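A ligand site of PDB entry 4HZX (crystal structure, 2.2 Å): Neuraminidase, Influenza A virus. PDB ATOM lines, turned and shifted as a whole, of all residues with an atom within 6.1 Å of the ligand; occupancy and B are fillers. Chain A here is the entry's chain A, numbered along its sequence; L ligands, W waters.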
ATOM      1  N   ARG A  37      -0.344  17.239 -13.709  1.00  0.00           N
ATOM      2  CA  ARG A  37      -1.707  17.312 -13.179  1.00  0.00           C
ATOM      3  C   ARG A  37      -2.575  18.056 -14.179  1.00  0.00           C
ATOM      4  O   ARG A  37      -2.104  18.488 -15.228  1.00  0.00           O
ATOM      5  CB  ARG A  37      -1.768  17.965 -11.791  1.00  0.00           C
ATOM      6  CG  ARG A  37      -1.976  16.960 -10.644  1.00  0.00           C
ATOM      7  CD  ARG A  37      -2.815  17.537  -9.501  1.00  0.00           C
ATOM      8  NE  ARG A  37      -4.228  17.625  -9.864  1.00  0.00           N
ATOM      9  CZ  ARG A  37      -5.114  18.432  -9.271  1.00  0.00           C
ATOM     10  NH1 ARG A  37      -4.748  19.229  -8.282  1.00  0.00           N
ATOM     11  NH2 ARG A  37      -6.372  18.435  -9.689  1.00  0.00           N
ATOM     12  N   GLU A  38      -3.861  18.194 -13.856  1.00  0.00           N
ATOM     13  CA  GLU A  38      -4.843  18.792 -14.767  1.00  0.00           C
ATOM     14  C   GLU A  38      -4.715  18.229 -16.177  1.00  0.00           C
ATOM     15  O   GLU A  38      -4.513  18.990 -17.131  1.00  0.00           O
ATOM     16  CB  GLU A  38      -4.703  20.314 -14.798  1.00  0.00           C
ATOM     17  CG  GLU A  38      -4.950  21.002 -13.467  1.00  0.00           C
ATOM     18  CD  GLU A  38      -3.739  20.959 -12.551  1.00  0.00           C
ATOM     19  OE1 GLU A  38      -2.609  20.843 -13.055  1.00  0.00           O
ATOM     20  OE2 GLU A  38      -3.938  21.048 -11.321  1.00  0.00           O
ATOM     21  N   LEU A  53      -0.742  19.510 -17.685  1.00  0.00           N
ATOM     22  CA  LEU A  53       0.188  20.509 -17.185  1.00  0.00           C
ATOM     23  C   LEU A  53       1.346  19.817 -16.469  1.00  0.00           C
ATOM     24  O   LEU A  53       1.182  19.292 -15.370  1.00  0.00           O
ATOM     25  CB  LEU A  53      -0.514  21.489 -16.248  1.00  0.00           C
ATOM     26  CG  LEU A  53      -1.607  22.359 -16.893  1.00  0.00           C
ATOM     27  CD1 LEU A  53      -2.287  23.227 -15.858  1.00  0.00           C
ATOM     28  CD2 LEU A  53      -1.018  23.224 -18.017  1.00  0.00           C
ATOM     29  N   ASP A  70       0.396  24.760  -7.193  1.00  0.00           N
ATOM     30  CA  ASP A  70      -0.397  24.894  -8.425  1.00  0.00           C
ATOM     31  C   ASP A  70       0.299  25.641  -9.553  1.00  0.00           C
ATOM     32  O   ASP A  70       0.283  25.199 -10.697  1.00  0.00           O
ATOM     33  CB  ASP A  70      -1.738  25.559  -8.120  1.00  0.00           C
ATOM     34  CG  ASP A  70      -2.651  24.699  -7.268  1.00  0.00           C
ATOM     35  OD1 ASP A  70      -3.214  23.724  -7.811  1.00  0.00           O
ATOM     36  OD2 ASP A  70      -2.800  24.987  -6.068  1.00  0.00           O
ATOM     37  N   ARG A  71       0.905  26.776  -9.244  1.00  0.00           N
ATOM     38  CA  ARG A  71       1.445  27.630 -10.299  1.00  0.00           C
ATOM     39  C   ARG A  71       2.926  27.934 -10.099  1.00  0.00           C
ATOM     40  O   ARG A  71       3.328  28.525  -9.101  1.00  0.00           O
ATOM     41  CB  ARG A  71       0.622  28.928 -10.393  1.00  0.00           C
ATOM     42  CG  ARG A  71      -0.883  28.668 -10.523  1.00  0.00           C
ATOM     43  CD  ARG A  71      -1.701  29.950 -10.417  1.00  0.00           C
ATOM     44  NE  ARG A  71      -1.566  30.587  -9.110  1.00  0.00           N
ATOM     45  CZ  ARG A  71      -2.152  30.155  -8.002  1.00  0.00           C
ATOM     46  NH1 ARG A  71      -1.967  30.793  -6.858  1.00  0.00           N
ATOM     47  NH2 ARG A  71      -2.916  29.069  -8.034  1.00  0.00           N
ATOM     48  N   ARG A  75       6.017  24.974 -15.225  1.00  0.00           N
ATOM     49  CA  ARG A  75       4.931  24.173 -15.756  1.00  0.00           C
ATOM     50  C   ARG A  75       4.678  24.539 -17.214  1.00  0.00           C
ATOM     51  O   ARG A  75       4.649  25.724 -17.582  1.00  0.00           O
ATOM     52  CB  ARG A  75       3.650  24.391 -14.942  1.00  0.00           C
ATOM     53  CG  ARG A  75       3.840  24.199 -13.452  1.00  0.00           C
ATOM     54  CD  ARG A  75       2.507  23.923 -12.775  1.00  0.00           C
ATOM     55  NE  ARG A  75       2.000  22.595 -13.105  1.00  0.00           N
ATOM     56  CZ  ARG A  75       0.855  22.097 -12.650  1.00  0.00           C
ATOM     57  NH1 ARG A  75       0.099  22.839 -11.841  1.00  0.00           N
ATOM     58  NH2 ARG A  75       0.462  20.882 -12.986  1.00  0.00           N
ATOM     59  N   TRP A  98       0.389  27.308 -16.494  1.00  0.00           N
ATOM     60  CA  TRP A  98      -0.163  26.658 -15.310  1.00  0.00           C
ATOM     61  C   TRP A  98      -1.701  26.579 -15.364  1.00  0.00           C
ATOM     62  O   TRP A  98      -2.366  26.298 -14.372  1.00  0.00           O
ATOM     63  CB  TRP A  98       0.316  27.274 -13.988  1.00  0.00           C
ATOM     64  CG  TRP A  98       0.422  28.787 -13.924  1.00  0.00           C
ATOM     65  CD1 TRP A  98       1.567  29.522 -13.833  1.00  0.00           C
ATOM     66  CD2 TRP A  98      -0.661  29.732 -13.886  1.00  0.00           C
ATOM     67  NE1 TRP A  98       1.281  30.858 -13.753  1.00  0.00           N
ATOM     68  CE2 TRP A  98      -0.081  31.016 -13.789  1.00  0.00           C
ATOM     69  CE3 TRP A  98      -2.045  29.623 -13.935  1.00  0.00           C
ATOM     70  CZ2 TRP A  98      -0.852  32.187 -13.747  1.00  0.00           C
ATOM     71  CZ3 TRP A  98      -2.815  30.782 -13.884  1.00  0.00           C
ATOM     72  CH2 TRP A  98      -2.212  32.044 -13.794  1.00  0.00           C
ATOM     73  N   SER A  99      -2.248  26.827 -16.554  1.00  0.00           N
ATOM     74  CA  SER A  99      -3.663  26.648 -16.823  1.00  0.00           C
ATOM     75  C   SER A  99      -3.816  26.633 -18.340  1.00  0.00           C
ATOM     76  O   SER A  99      -3.163  27.416 -19.022  1.00  0.00           O
ATOM     77  CB  SER A  99      -4.479  27.788 -16.225  1.00  0.00           C
ATOM     78  OG  SER A  99      -5.871  27.563 -16.403  1.00  0.00           O
ATOM     79  N   ILE A 142      -5.155  35.733 -10.893  1.00  0.00           N
ATOM     80  CA  ILE A 142      -5.012  34.361 -11.393  1.00  0.00           C
ATOM     81  C   ILE A 142      -5.914  34.102 -12.602  1.00  0.00           C
ATOM     82  O   ILE A 142      -6.814  33.259 -12.548  1.00  0.00           O
ATOM     83  CB  ILE A 142      -5.293  33.314 -10.289  1.00  0.00           C
ATOM     84  CG1 ILE A 142      -4.522  33.645  -9.018  1.00  0.00           C
ATOM     85  CG2 ILE A 142      -4.933  31.926 -10.777  1.00  0.00           C
ATOM     86  CD1 ILE A 142      -4.849  32.731  -7.844  1.00  0.00           C
ATOM     87  N   LEU A 143      -5.681  34.850 -13.679  1.00  0.00           N
ATOM     88  CA  LEU A 143      -6.320  34.555 -14.951  1.00  0.00           C
ATOM     89  C   LEU A 143      -6.155  33.058 -15.241  1.00  0.00           C
ATOM     90  O   LEU A 143      -5.041  32.519 -15.154  1.00  0.00           O
ATOM     91  CB  LEU A 143      -5.674  35.381 -16.056  1.00  0.00           C
ATOM     92  CG  LEU A 143      -6.178  35.200 -17.483  1.00  0.00           C
ATOM     93  CD1 LEU A 143      -7.634  35.627 -17.585  1.00  0.00           C
ATOM     94  CD2 LEU A 143      -5.310  35.984 -18.470  1.00  0.00           C
ATOM     95  N   ARG A 144      -7.256  32.384 -15.570  1.00  0.00           N
ATOM     96  CA  ARG A 144      -7.245  30.925 -15.691  1.00  0.00           C
ATOM     97  C   ARG A 144      -8.340  30.413 -16.614  1.00  0.00           C
ATOM     98  O   ARG A 144      -9.260  31.162 -16.975  1.00  0.00           O
ATOM     99  CB  ARG A 144      -7.375  30.279 -14.306  1.00  0.00           C
ATOM    100  CG  ARG A 144      -8.601  30.738 -13.526  1.00  0.00           C
ATOM    101  CD  ARG A 144      -8.478  30.379 -12.058  1.00  0.00           C
ATOM    102  NE  ARG A 144      -9.672  30.756 -11.305  1.00  0.00           N
ATOM    103  CZ  ARG A 144      -9.858  31.959 -10.746  1.00  0.00           C
ATOM    104  NH1 ARG A 144      -8.926  32.888 -10.875  1.00  0.00           N
ATOM    105  NH2 ARG A 144     -10.973  32.210 -10.078  1.00  0.00           N
ATOM    106  N   GLU A 147      -8.897  23.733 -18.337  1.00  0.00           N
ATOM    107  CA  GLU A 147      -8.176  22.491 -18.002  1.00  0.00           C
ATOM    108  C   GLU A 147      -8.779  21.294 -18.744  1.00  0.00           C
ATOM    109  O   GLU A 147      -8.632  20.151 -18.322  1.00  0.00           O
ATOM    110  CB  GLU A 147      -8.147  22.211 -16.500  1.00  0.00           C
ATOM    111  CG  GLU A 147      -7.936  23.440 -15.596  1.00  0.00           C
ATOM    112  CD  GLU A 147      -6.605  24.144 -15.791  1.00  0.00           C
ATOM    113  OE1 GLU A 147      -5.824  23.736 -16.688  1.00  0.00           O
ATOM    114  OE2 GLU A 147      -6.339  25.115 -15.051  1.00  0.00           O
ATOM    115  N   GLY A 164     -10.368  36.330 -11.075  1.00  0.00           N
ATOM    116  CA  GLY A 164     -10.961  36.798  -9.844  1.00  0.00           C
ATOM    117  C   GLY A 164     -10.838  35.800  -8.703  1.00  0.00           C
ATOM    118  O   GLY A 164     -10.165  34.789  -8.838  1.00  0.00           O
ATOM    119  N   ALA A 166     -11.340  32.827  -6.007  1.00  0.00           N
ATOM    120  CA  ALA A 166     -11.706  31.430  -6.184  1.00  0.00           C
ATOM    121  C   ALA A 166     -12.886  31.031  -5.294  1.00  0.00           C
ATOM    122  O   ALA A 166     -13.552  30.024  -5.552  1.00  0.00           O
ATOM    123  CB  ALA A 166     -10.508  30.536  -5.899  1.00  0.00           C
ATOM    124  N   HIS A 195     -20.802  31.630  -9.825  1.00  0.00           N
ATOM    125  CA  HIS A 195     -19.388  31.303  -9.825  1.00  0.00           C
ATOM    126  C   HIS A 195     -19.107  30.262 -10.896  1.00  0.00           C
ATOM    127  O   HIS A 195     -19.886  29.330 -11.088  1.00  0.00           O
ATOM    128  CB  HIS A 195     -18.930  30.785  -8.453  1.00  0.00           C
ATOM    129  CG  HIS A 195     -17.452  30.835  -8.249  1.00  0.00           C
ATOM    130  ND1 HIS A 195     -16.774  32.014  -7.999  1.00  0.00           N
ATOM    131  CD2 HIS A 195     -16.512  29.860  -8.291  1.00  0.00           C
ATOM    132  CE1 HIS A 195     -15.479  31.754  -7.875  1.00  0.00           C
ATOM    133  NE2 HIS A 195     -15.294  30.457  -8.042  1.00  0.00           N
ATOM    134  N   GLU A 197     -15.835  28.001 -12.878  1.00  0.00           N
ATOM    135  CA  GLU A 197     -14.452  27.569 -13.028  1.00  0.00           C
ATOM    136  C   GLU A 197     -14.388  26.318 -13.905  1.00  0.00           C
ATOM    137  O   GLU A 197     -15.359  25.567 -14.009  1.00  0.00           O
ATOM    138  CB  GLU A 197     -13.851  27.225 -11.661  1.00  0.00           C
ATOM    139  CG  GLU A 197     -14.009  28.319 -10.615  1.00  0.00           C
ATOM    140  CD  GLU A 197     -12.878  29.328 -10.629  1.00  0.00           C
ATOM    141  OE1 GLU A 197     -12.916  30.290  -9.840  1.00  0.00           O
ATOM    142  OE2 GLU A 197     -11.938  29.142 -11.422  1.00  0.00           O
ATOM    143  N   GLU A 198     -13.234  26.115 -14.547  1.00  0.00           N
ATOM    144  CA  GLU A 198     -12.881  24.832 -15.165  1.00  0.00           C
ATOM    145  C   GLU A 198     -14.011  24.167 -15.949  1.00  0.00           C
ATOM    146  O   GLU A 198     -14.390  23.025 -15.673  1.00  0.00           O
ATOM    147  CB  GLU A 198     -12.327  23.893 -14.091  1.00  0.00           C
ATOM    148  CG  GLU A 198     -11.051  24.423 -13.439  1.00  0.00           C
ATOM    149  CD  GLU A 198     -10.732  23.717 -12.126  1.00  0.00           C
ATOM    150  OE1 GLU A 198     -11.657  23.144 -11.528  1.00  0.00           O
ATOM    151  OE2 GLU A 198      -9.543  23.737 -11.713  1.00  0.00           O
ATOM    152  N   ARG A 212     -17.656  24.271 -12.864  1.00  0.00           N
ATOM    153  CA  ARG A 212     -17.454  24.142 -11.422  1.00  0.00           C
ATOM    154  C   ARG A 212     -17.728  25.474 -10.716  1.00  0.00           C
ATOM    155  O   ARG A 212     -17.075  26.473 -10.996  1.00  0.00           O
ATOM    156  CB  ARG A 212     -16.023  23.680 -11.132  1.00  0.00           C
ATOM    157  CG  ARG A 212     -15.538  23.869  -9.704  1.00  0.00           C
ATOM    158  CD  ARG A 212     -14.111  23.367  -9.572  1.00  0.00           C
ATOM    159  NE  ARG A 212     -13.462  23.780  -8.332  1.00  0.00           N
ATOM    160  CZ  ARG A 212     -12.230  23.413  -7.984  1.00  0.00           C
ATOM    161  NH1 ARG A 212     -11.519  22.627  -8.771  1.00  0.00           N
ATOM    162  NH2 ARG A 212     -11.703  23.831  -6.842  1.00  0.00           N
ATOM    163  N   ASN A 214     -17.208  27.207  -7.407  1.00  0.00           N
ATOM    164  CA  ASN A 214     -16.325  26.942  -6.278  1.00  0.00           C
ATOM    165  C   ASN A 214     -16.740  27.690  -5.018  1.00  0.00           C
ATOM    166  O   ASN A 214     -15.995  27.738  -4.038  1.00  0.00           O
ATOM    167  CB  ASN A 214     -14.880  27.305  -6.644  1.00  0.00           C
ATOM    168  CG  ASN A 214     -13.859  26.523  -5.836  1.00  0.00           C
ATOM    169  OD1 ASN A 214     -13.977  25.301  -5.713  1.00  0.00           O
ATOM    170  ND2 ASN A 214     -12.881  27.220  -5.277  1.00  0.00           N
ATOM    171  N   GLY A 266     -14.856  22.642  -4.449  1.00  0.00           N
ATOM    172  CA  GLY A 266     -15.378  21.978  -5.623  1.00  0.00           C
ATOM    173  C   GLY A 266     -14.327  21.159  -6.350  1.00  0.00           C
ATOM    174  O   GLY A 266     -13.181  21.055  -5.913  1.00  0.00           O
ATOM    175  N   VAL A 267     -14.722  20.567  -7.478  1.00  0.00           N
ATOM    176  CA  VAL A 267     -13.822  19.801  -8.322  1.00  0.00           C
ATOM    177  C   VAL A 267     -14.278  19.920  -9.775  1.00  0.00           C
ATOM    178  O   VAL A 267     -15.475  20.001 -10.054  1.00  0.00           O
ATOM    179  CB  VAL A 267     -13.783  18.310  -7.912  1.00  0.00           C
ATOM    180  CG1 VAL A 267     -15.047  17.594  -8.364  1.00  0.00           C
ATOM    181  CG2 VAL A 267     -12.549  17.611  -8.459  1.00  0.00           C
ATOM    182  N   ARG A 289     -12.162  13.301  -2.877  1.00  0.00           N
ATOM    183  CA  ARG A 289     -11.883  12.976  -4.267  1.00  0.00           C
ATOM    184  C   ARG A 289     -11.494  11.514  -4.432  1.00  0.00           C
ATOM    185  O   ARG A 289     -10.406  11.184  -4.923  1.00  0.00           O
ATOM    186  CB  ARG A 289     -10.804  13.907  -4.829  1.00  0.00           C
ATOM    187  CG  ARG A 289     -11.258  15.349  -4.913  1.00  0.00           C
ATOM    188  CD  ARG A 289     -10.153  16.276  -5.350  1.00  0.00           C
ATOM    189  NE  ARG A 289     -10.667  17.637  -5.528  1.00  0.00           N
ATOM    190  CZ  ARG A 289      -9.946  18.661  -5.940  1.00  0.00           C
ATOM    191  NH1 ARG A 289      -8.650  18.507  -6.215  1.00  0.00           N
ATOM    192  NH2 ARG A 289     -10.504  19.854  -6.082  1.00  0.00           N
ATOM    193  N   TYR A 324      -9.888  15.265 -11.038  1.00  0.00           N
ATOM    194  CA  TYR A 324     -10.600  15.969 -12.105  1.00  0.00           C
ATOM    195  C   TYR A 324     -11.213  15.014 -13.125  1.00  0.00           C
ATOM    196  O   TYR A 324     -10.777  13.872 -13.253  1.00  0.00           O
ATOM    197  CB  TYR A 324      -9.675  16.943 -12.842  1.00  0.00           C
ATOM    198  CG  TYR A 324      -9.466  18.265 -12.131  1.00  0.00           C
ATOM    199  CD1 TYR A 324      -9.879  18.445 -10.825  1.00  0.00           C
ATOM    200  CD2 TYR A 324      -8.857  19.324 -12.787  1.00  0.00           C
ATOM    201  CE1 TYR A 324      -9.689  19.643 -10.172  1.00  0.00           C
ATOM    202  CE2 TYR A 324      -8.664  20.532 -12.156  1.00  0.00           C
ATOM    203  CZ  TYR A 324      -9.081  20.692 -10.842  1.00  0.00           C
ATOM    204  OH  TYR A 324      -8.887  21.888 -10.202  1.00  0.00           O
ATOM    205  N   ILE A 345      -5.476  11.155  -9.174  1.00  0.00           N
ATOM    206  CA  ILE A 345      -4.422  11.868  -8.466  1.00  0.00           C
ATOM    207  C   ILE A 345      -3.755  11.009  -7.394  1.00  0.00           C
ATOM    208  O   ILE A 345      -4.423  10.430  -6.547  1.00  0.00           O
ATOM    209  CB  ILE A 345      -4.973  13.146  -7.794  1.00  0.00           C
ATOM    210  CG1 ILE A 345      -5.698  14.022  -8.809  1.00  0.00           C
ATOM    211  CG2 ILE A 345      -3.857  13.919  -7.113  1.00  0.00           C
ATOM    212  CD1 ILE A 345      -6.381  15.231  -8.215  1.00  0.00           C
HETATM  213  C1  LIG L   1      -7.915  21.810  -7.342  1.00  0.00           C
HETATM  214  O1  LIG L   1      -7.384  20.723  -7.481  1.00  0.00           O
HETATM  215  O2  LIG L   1      -9.062  21.920  -6.578  1.00  0.00           O
HETATM  216  C2  LIG L   1      -7.323  23.022  -7.996  1.00  0.00           C
HETATM  217  C3  LIG L   1      -5.933  22.961  -8.675  1.00  0.00           C
HETATM  218  C4  LIG L   1      -5.749  23.812  -9.907  1.00  0.00           C
HETATM  219  C5  LIG L   1      -6.331  25.225  -9.887  1.00  0.00           C
HETATM  220  N1  LIG L   1      -6.026  26.160 -10.951  1.00  0.00           N
HETATM  221  C6  LIG L   1      -4.902  27.026 -10.849  1.00  0.00           C
HETATM  222  O3  LIG L   1      -4.183  26.975  -9.858  1.00  0.00           O
HETATM  223  C7  LIG L   1      -4.587  27.989 -11.957  1.00  0.00           C
HETATM  224  C8  LIG L   1      -7.561  25.484  -8.984  1.00  0.00           C
HETATM  225  C9  LIG L   1      -8.211  24.276  -8.242  1.00  0.00           C
HETATM  226  O4  LIG L   1      -7.819  26.778  -8.527  1.00  0.00           O
HETATM  227  C10 LIG L   1      -8.627  27.634  -9.275  1.00  0.00           C
HETATM  228  C11 LIG L   1     -10.021  27.111  -9.495  1.00  0.00           C
HETATM  229  C12 LIG L   1      -8.598  29.068  -8.812  1.00  0.00           C
HETATM  230  C13 LIG L   1      -7.254  29.693  -8.585  1.00  0.00           C
HETATM  231  C14 LIG L   1     -10.860  26.843  -8.284  1.00  0.00           C
HETATM  232  N2  LIG L   1      -4.654  23.518 -10.795  1.00  0.00           N
HETATM  233  O   HOH W   1      -7.653  25.418 -12.884  1.00  0.00           O
HETATM  234  O   HOH W   2      -7.563  26.403  -5.690  1.00  0.00           O
HETATM  235  O   HOH W   3      -4.348  24.637 -13.080  1.00  0.00           O
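The guanidinium group (NH2) of Arg 289 is in salt-bridge range of an oxygen (O2) of the ligand (2.6 Å). The guanidinium group of Arg 71 is in hydrogen-bond range of an oxygen (O3) of the ligand (3.1 Å). A nitrogen (N2) of the ligand lies within salt-bridge range of the side-chain carboxylate (OD1) of Asp 70, 3.3 Å away. The side-chain hydroxyl (OH) of Tyr 324 lies close to an oxygen (O1) of the ligand (3.3 Å). NH1 of Arg 37 is in salt-bridge range of O1 of the ligand, at 3.1 Å. OE2 of Glu 38 lies within salt-bridge range of N2 of the ligand. O2 of the ligand lies within salt-bridge range of NH2 of Arg 212 (3.3 Å).
NH1 of Arg 212 is in hydrogen-bond range of OH of Tyr 324 (3.1 Å). A ring nitrogen (NE2) of His 195 lies within hydrogen-bond range of the backbone carbonyl oxygen (O) of Ala 166 (3.1 Å). The backbone NH of Leu 53 is in hydrogen-bond range of the backbone carbonyl oxygen of Arg 37 (3.0 Å). The guanidinium group of Arg 144 lies within hydrogen-bond range of the backbone carbonyl oxygen of Gly 164 (3.0 Å). The guanidinium group (NH2) of Arg 212 is in hydrogen-bond range of the backbone carbonyl oxygen (O) of Gly 266, 3.3 Å away. NH1 of Arg 212 lies within salt-bridge range of OE1 of Glu 198. OE2 of Glu 38 is in salt-bridge range of NH1 of Arg 37, 3.6 Å away. The backbone carbonyl oxygen (O) of Asp 70 lies within hydrogen-bond range of the guanidinium group (NH1) of Arg 75 (2.6 Å).
CE3 of Trp 98 touches C7 of the ligand, at 3.6 Å. Ile 142 touches the ligand. Arg 144 touches the ligand. Ala 166 touches the ligand. Glu 197 touches the ligand (OE2 to C11, 3.4 Å). OE2 of Glu 198 touches C9 of the ligand (3.8 Å). Asn 214 touches the ligand (ND2 to C14, 3.6 Å). Hydrophobic or aromatic side chains within 4 Å of the ligand: Trp 98, Ile 142, Ala 166 and Tyr 324. 14 residues have an atom within 4 Å of the ligand: Arg 37, Glu 38, Asp 70, Arg 71, Trp 98, Ile 142, Arg 144, Ala 166, Glu 197, Glu 198, Arg 212, Asn 214, Arg 289 and Tyr 324. The nearest printed residue that does not touch the ligand is Glu 147 (4.2 Å).
Water W3 lies within hydrogen-bond range of a nitrogen (N2) of the ligand (2.6 Å), the side-chain carboxylate of Glu 147 (2.8 Å) and the backbone carbonyl oxygen of Trp 98 (2.9 Å). Water W1 lies within hydrogen-bond range of OE2 of Glu 147, N1 of the ligand and OE2 of Glu 198.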
